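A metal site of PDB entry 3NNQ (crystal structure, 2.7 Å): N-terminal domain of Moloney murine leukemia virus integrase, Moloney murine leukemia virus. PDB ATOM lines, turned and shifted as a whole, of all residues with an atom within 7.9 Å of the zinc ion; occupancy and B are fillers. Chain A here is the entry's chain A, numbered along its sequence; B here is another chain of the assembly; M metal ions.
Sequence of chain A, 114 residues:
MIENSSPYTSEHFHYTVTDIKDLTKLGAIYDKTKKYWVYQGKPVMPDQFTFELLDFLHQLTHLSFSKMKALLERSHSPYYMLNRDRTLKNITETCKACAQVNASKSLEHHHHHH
O of Leu 63 sits at hydrogen-bond distance from ND1 of His 58 (3.0 Å). NE2 of His 62 sits at hydrogen-bond distance from O of Gln 59 of chain A (3.1 Å). NE2 of His 62 is in hydrogen-bond range of O of Gln 59 of chain B (2.8 Å). The side-chain sulfur of Cys 95 sits close to the backbone NH of Ala 97 (3.6 Å).
Within 4 Å of the zinc ion: His 58, His 62, Cys 95 and Cys 98. The nearest printed residue that does not touch the zinc ion is Ala 97 (4.5 Å).
The zinc ion is bound by a ring nitrogen (NE2) of His 58 (2.1 Å), a ring nitrogen (ND1) of His 62 (2.1 Å), the side-chain sulfur (SG) of Cys 95 (2.3 Å) and the side-chain sulfur (SG) of Cys 98 (2.3 Å). The zinc ion has four donor atoms within binding distance.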
ATOM      1  N   ASP A  55     -34.730 -21.519  19.636  1.00  0.00           N
ATOM      2  CA  ASP A  55     -34.847 -21.076  18.255  1.00  0.00           C
ATOM      3  C   ASP A  55     -35.565 -19.728  18.237  1.00  0.00           C
ATOM      4  O   ASP A  55     -35.122 -18.792  17.566  1.00  0.00           O
ATOM      5  CB  ASP A  55     -35.628 -22.098  17.428  1.00  0.00           C
ATOM      6  CG  ASP A  55     -35.942 -21.591  16.036  1.00  0.00           C
ATOM      7  OD1 ASP A  55     -35.151 -21.886  15.106  1.00  0.00           O
ATOM      8  OD2 ASP A  55     -36.971 -20.908  15.865  1.00  0.00           O
ATOM      9  N   LEU A  57     -35.865 -17.498  20.592  1.00  0.00           N
ATOM     10  CA  LEU A  57     -35.005 -16.467  21.125  1.00  0.00           C
ATOM     11  C   LEU A  57     -33.957 -16.020  20.110  1.00  0.00           C
ATOM     12  O   LEU A  57     -33.686 -14.820  19.982  1.00  0.00           O
ATOM     13  CB  LEU A  57     -34.329 -16.934  22.412  1.00  0.00           C
ATOM     14  CG  LEU A  57     -35.338 -17.138  23.538  1.00  0.00           C
ATOM     15  CD1 LEU A  57     -34.653 -17.554  24.821  1.00  0.00           C
ATOM     16  CD2 LEU A  57     -36.152 -15.872  23.745  1.00  0.00           C
ATOM     17  N   HIS A  58     -33.368 -16.973  19.395  1.00  0.00           N
ATOM     18  CA  HIS A  58     -32.329 -16.620  18.431  1.00  0.00           C
ATOM     19  C   HIS A  58     -32.894 -15.808  17.269  1.00  0.00           C
ATOM     20  O   HIS A  58     -32.246 -14.888  16.766  1.00  0.00           O
ATOM     21  CB  HIS A  58     -31.601 -17.846  17.899  1.00  0.00           C
ATOM     22  CG  HIS A  58     -30.485 -17.491  16.964  1.00  0.00           C
ATOM     23  ND1 HIS A  58     -29.263 -17.021  17.408  1.00  0.00           N
ATOM     24  CD2 HIS A  58     -30.407 -17.509  15.615  1.00  0.00           C
ATOM     25  CE1 HIS A  58     -28.484 -16.775  16.369  1.00  0.00           C
ATOM     26  NE2 HIS A  58     -29.157 -17.064  15.266  1.00  0.00           N
ATOM     27  N   GLN A  59     -34.100 -16.162  16.848  1.00  0.00           N
ATOM     28  CA  GLN A  59     -34.764 -15.451  15.759  1.00  0.00           C
ATOM     29  C   GLN A  59     -34.942 -13.964  16.074  1.00  0.00           C
ATOM     30  O   GLN A  59     -34.833 -13.123  15.191  1.00  0.00           O
ATOM     31  CB  GLN A  59     -36.109 -16.099  15.469  1.00  0.00           C
ATOM     32  CG  GLN A  59     -35.973 -17.490  14.894  1.00  0.00           C
ATOM     33  CD  GLN A  59     -35.201 -17.465  13.601  1.00  0.00           C
ATOM     34  OE1 GLN A  59     -35.381 -16.581  12.768  1.00  0.00           O
ATOM     35  NE2 GLN A  59     -34.325 -18.451  13.425  1.00  0.00           N
ATOM     36  N   LEU A  60     -35.194 -13.658  17.347  1.00  0.00           N
ATOM     37  CA  LEU A  60     -35.498 -12.287  17.754  1.00  0.00           C
ATOM     38  C   LEU A  60     -34.255 -11.456  18.054  1.00  0.00           C
ATOM     39  O   LEU A  60     -34.291 -10.232  17.984  1.00  0.00           O
ATOM     40  CB  LEU A  60     -36.432 -12.273  18.961  1.00  0.00           C
ATOM     41  CG  LEU A  60     -37.831 -12.863  18.761  1.00  0.00           C
ATOM     42  CD1 LEU A  60     -38.623 -12.708  20.045  1.00  0.00           C
ATOM     43  CD2 LEU A  60     -38.559 -12.199  17.607  1.00  0.00           C
ATOM     44  N   THR A  61     -33.154 -12.125  18.402  1.00  0.00           N
ATOM     45  CA  THR A  61     -31.952 -11.419  18.797  1.00  0.00           C
ATOM     46  C   THR A  61     -30.778 -11.743  17.892  1.00  0.00           C
ATOM     47  O   THR A  61     -29.886 -10.922  17.695  1.00  0.00           O
ATOM     48  CB  THR A  61     -31.552 -11.759  20.243  1.00  0.00           C
ATOM     49  OG1 THR A  61     -31.212 -13.147  20.326  1.00  0.00           O
ATOM     50  CG2 THR A  61     -32.685 -11.456  21.192  1.00  0.00           C
ATOM     51  N   HIS A  62     -30.772 -12.960  17.362  1.00  0.00           N
ATOM     52  CA  HIS A  62     -29.675 -13.457  16.553  1.00  0.00           C
ATOM     53  C   HIS A  62     -28.343 -13.317  17.269  1.00  0.00           C
ATOM     54  O   HIS A  62     -27.297 -13.172  16.634  1.00  0.00           O
ATOM     55  CB  HIS A  62     -29.662 -12.789  15.176  1.00  0.00           C
ATOM     56  CG  HIS A  62     -30.766 -13.272  14.285  1.00  0.00           C
ATOM     57  ND1 HIS A  62     -30.670 -14.455  13.572  1.00  0.00           N
ATOM     58  CD2 HIS A  62     -31.981 -12.759  14.010  1.00  0.00           C
ATOM     59  CE1 HIS A  62     -31.791 -14.641  12.891  1.00  0.00           C
ATOM     60  NE2 HIS A  62     -32.609 -13.629  13.141  1.00  0.00           N
ATOM     61  N   LEU A  63     -28.388 -13.384  18.590  1.00  0.00           N
ATOM     62  CA  LEU A  63     -27.194 -13.423  19.420  1.00  0.00           C
ATOM     63  C   LEU A  63     -26.389 -14.692  19.163  1.00  0.00           C
ATOM     64  O   LEU A  63     -26.944 -15.751  18.848  1.00  0.00           O
ATOM     65  CB  LEU A  63     -27.588 -13.369  20.892  1.00  0.00           C
ATOM     66  CG  LEU A  63     -28.182 -12.028  21.320  1.00  0.00           C
ATOM     67  CD1 LEU A  63     -28.855 -12.153  22.674  1.00  0.00           C
ATOM     68  CD2 LEU A  63     -27.096 -10.968  21.361  1.00  0.00           C
ATOM     69  N   SER A  64     -25.070 -14.586  19.318  1.00  0.00           N
ATOM     70  CA  SER A  64     -24.176 -15.711  19.069  1.00  0.00           C
ATOM     71  C   SER A  64     -24.328 -16.800  20.118  1.00  0.00           C
ATOM     72  O   SER A  64     -25.055 -16.635  21.107  1.00  0.00           O
ATOM     73  CB  SER A  64     -22.715 -15.244  18.992  1.00  0.00           C
ATOM     74  OG  SER A  64     -22.245 -14.777  20.253  1.00  0.00           O
ATOM     75  N   MET A  68     -25.785 -16.006  23.936  1.00  0.00           N
ATOM     76  CA  MET A  68     -27.015 -16.549  24.492  1.00  0.00           C
ATOM     77  C   MET A  68     -26.730 -17.456  25.688  1.00  0.00           C
ATOM     78  O   MET A  68     -27.373 -17.347  26.734  1.00  0.00           O
ATOM     79  CB  MET A  68     -27.821 -17.304  23.436  1.00  0.00           C
ATOM     80  CG  MET A  68     -28.598 -16.401  22.499  1.00  0.00           C
ATOM     81  SD  MET A  68     -29.557 -17.303  21.278  1.00  0.00           S
ATOM     82  CE  MET A  68     -30.819 -18.029  22.309  1.00  0.00           C
ATOM     83  N   ILE A  91     -28.664 -24.346  16.273  1.00  0.00           N
ATOM     84  CA  ILE A  91     -29.459 -23.201  15.853  1.00  0.00           C
ATOM     85  C   ILE A  91     -28.595 -22.078  15.281  1.00  0.00           C
ATOM     86  O   ILE A  91     -28.838 -21.595  14.173  1.00  0.00           O
ATOM     87  CB  ILE A  91     -30.296 -22.660  17.028  1.00  0.00           C
ATOM     88  CG1 ILE A  91     -31.404 -23.647  17.386  1.00  0.00           C
ATOM     89  CG2 ILE A  91     -30.873 -21.287  16.707  1.00  0.00           C
ATOM     90  CD1 ILE A  91     -32.145 -23.320  18.662  1.00  0.00           C
ATOM     91  N   THR A  92     -27.576 -21.692  16.039  1.00  0.00           N
ATOM     92  CA  THR A  92     -26.671 -20.620  15.635  1.00  0.00           C
ATOM     93  C   THR A  92     -25.864 -20.997  14.393  1.00  0.00           C
ATOM     94  O   THR A  92     -25.790 -20.228  13.426  1.00  0.00           O
ATOM     95  CB  THR A  92     -25.708 -20.243  16.784  1.00  0.00           C
ATOM     96  OG1 THR A  92     -24.888 -21.372  17.101  1.00  0.00           O
ATOM     97  CG2 THR A  92     -26.482 -19.837  18.027  1.00  0.00           C
ATOM     98  N   GLU A  93     -25.274 -22.186  14.424  1.00  0.00           N
ATOM     99  CA  GLU A  93     -24.454 -22.683  13.316  1.00  0.00           C
ATOM    100  C   GLU A  93     -25.211 -22.863  12.009  1.00  0.00           C
ATOM    101  O   GLU A  93     -24.610 -22.935  10.949  1.00  0.00           O
ATOM    102  CB  GLU A  93     -23.793 -24.019  13.702  1.00  0.00           C
ATOM    103  CG  GLU A  93     -22.732 -23.914  14.769  1.00  0.00           C
ATOM    104  CD  GLU A  93     -21.630 -22.939  14.390  1.00  0.00           C
ATOM    105  OE1 GLU A  93     -20.998 -23.122  13.334  1.00  0.00           O
ATOM    106  OE2 GLU A  93     -21.408 -21.977  15.159  1.00  0.00           O
ATOM    107  N   THR A  94     -26.536 -22.935  12.094  1.00  0.00           N
ATOM    108  CA  THR A  94     -27.338 -23.121  10.890  1.00  0.00           C
ATOM    109  C   THR A  94     -28.200 -21.904  10.566  1.00  0.00           C
ATOM    110  O   THR A  94     -28.954 -21.908   9.593  1.00  0.00           O
ATOM    111  CB  THR A  94     -28.257 -24.363  10.997  1.00  0.00           C
ATOM    112  OG1 THR A  94     -29.223 -24.164  12.031  1.00  0.00           O
ATOM    113  CG2 THR A  94     -27.431 -25.605  11.298  1.00  0.00           C
ATOM    114  N   CYS A  95     -28.088 -20.865  11.387  1.00  0.00           N
ATOM    115  CA  CYS A  95     -28.800 -19.624  11.100  1.00  0.00           C
ATOM    116  C   CYS A  95     -28.150 -18.915   9.917  1.00  0.00           C
ATOM    117  O   CYS A  95     -26.998 -18.487   9.993  1.00  0.00           O
ATOM    118  CB  CYS A  95     -28.812 -18.694  12.311  1.00  0.00           C
ATOM    119  SG  CYS A  95     -29.551 -17.095  11.961  1.00  0.00           S
ATOM    120  N   LYS A  96     -28.890 -18.809   8.822  1.00  0.00           N
ATOM    121  CA  LYS A  96     -28.371 -18.180   7.611  1.00  0.00           C
ATOM    122  C   LYS A  96     -28.202 -16.668   7.751  1.00  0.00           C
ATOM    123  O   LYS A  96     -27.317 -16.088   7.123  1.00  0.00           O
ATOM    124  CB  LYS A  96     -29.247 -18.525   6.394  1.00  0.00           C
ATOM    125  CG  LYS A  96     -29.287 -20.015   6.085  1.00  0.00           C
ATOM    126  CD  LYS A  96     -30.134 -20.318   4.863  1.00  0.00           C
ATOM    127  CE  LYS A  96     -30.152 -21.814   4.591  1.00  0.00           C
ATOM    128  NZ  LYS A  96     -30.965 -22.163   3.387  1.00  0.00           N
ATOM    129  N   ALA A  97     -29.040 -16.045   8.573  1.00  0.00           N
ATOM    130  CA  ALA A  97     -28.919 -14.611   8.811  1.00  0.00           C
ATOM    131  C   ALA A  97     -27.602 -14.323   9.501  1.00  0.00           C
ATOM    132  O   ALA A  97     -26.873 -13.406   9.133  1.00  0.00           O
ATOM    133  CB  ALA A  97     -30.078 -14.112   9.653  1.00  0.00           C
ATOM    134  N   CYS A  98     -27.298 -15.132  10.510  1.00  0.00           N
ATOM    135  CA  CYS A  98     -26.044 -15.024  11.237  1.00  0.00           C
ATOM    136  C   CYS A  98     -24.871 -15.305  10.286  1.00  0.00           C
ATOM    137  O   CYS A  98     -23.822 -14.686  10.386  1.00  0.00           O
ATOM    138  CB  CYS A  98     -26.022 -16.004  12.411  1.00  0.00           C
ATOM    139  SG  CYS A  98     -26.765 -15.350  13.929  1.00  0.00           S
ATOM    140  N   ALA A  99     -25.104 -16.237   9.369  1.00  0.00           N
ATOM    141  CA  ALA A  99     -24.093 -16.651   8.387  1.00  0.00           C
ATOM    142  C   ALA A  99     -23.717 -15.502   7.459  1.00  0.00           C
ATOM    143  O   ALA A  99     -22.548 -15.305   7.139  1.00  0.00           O
ATOM    144  CB  ALA A  99     -24.613 -17.835   7.577  1.00  0.00           C
ATOM    145  N   VAL A 101     -24.370 -12.092   8.030  1.00  0.00           N
ATOM    146  CA  VAL A 101     -23.785 -10.966   8.776  1.00  0.00           C
ATOM    147  C   VAL A 101     -22.335 -11.221   9.180  1.00  0.00           C
ATOM    148  O   VAL A 101     -21.663 -10.314   9.671  1.00  0.00           O
ATOM    149  CB  VAL A 101     -24.596 -10.620  10.058  1.00  0.00           C
ATOM    150  CG1 VAL A 101     -25.960 -10.071   9.699  1.00  0.00           C
ATOM    151  CG2 VAL A 101     -24.704 -11.829  10.968  1.00  0.00           C
ATOM    152  N   GLN B  59     -35.406 -11.049   9.177  1.00  0.00           N
ATOM    153  CA  GLN B  59     -34.739 -11.843  10.197  1.00  0.00           C
ATOM    154  C   GLN B  59     -34.145 -10.976  11.302  1.00  0.00           C
ATOM    155  O   GLN B  59     -34.153 -11.345  12.474  1.00  0.00           O
ATOM    156  CB  GLN B  59     -33.653 -12.700   9.558  1.00  0.00           C
ATOM    157  CG  GLN B  59     -34.222 -13.771   8.659  1.00  0.00           C
ATOM    158  CD  GLN B  59     -35.131 -14.707   9.409  1.00  0.00           C
ATOM    159  OE1 GLN B  59     -34.840 -15.089  10.549  1.00  0.00           O
ATOM    160  NE2 GLN B  59     -36.249 -15.081   8.798  1.00  0.00           N
ATOM    161  N   LEU B  60     -33.647  -9.802  10.919  1.00  0.00           N
ATOM    162  CA  LEU B  60     -32.953  -8.943  11.868  1.00  0.00           C
ATOM    163  C   LEU B  60     -33.887  -8.013  12.642  1.00  0.00           C
ATOM    164  O   LEU B  60     -33.546  -7.549  13.743  1.00  0.00           O
ATOM    165  CB  LEU B  60     -31.890  -8.102  11.148  1.00  0.00           C
ATOM    166  CG  LEU B  60     -30.736  -8.866  10.495  1.00  0.00           C
ATOM    167  CD1 LEU B  60     -29.765  -7.890   9.865  1.00  0.00           C
ATOM    168  CD2 LEU B  60     -30.026  -9.757  11.505  1.00  0.00           C
HETATM  169 ZN    ZN M   1     -29.053 -15.726  13.713  1.00  0.00          ZN
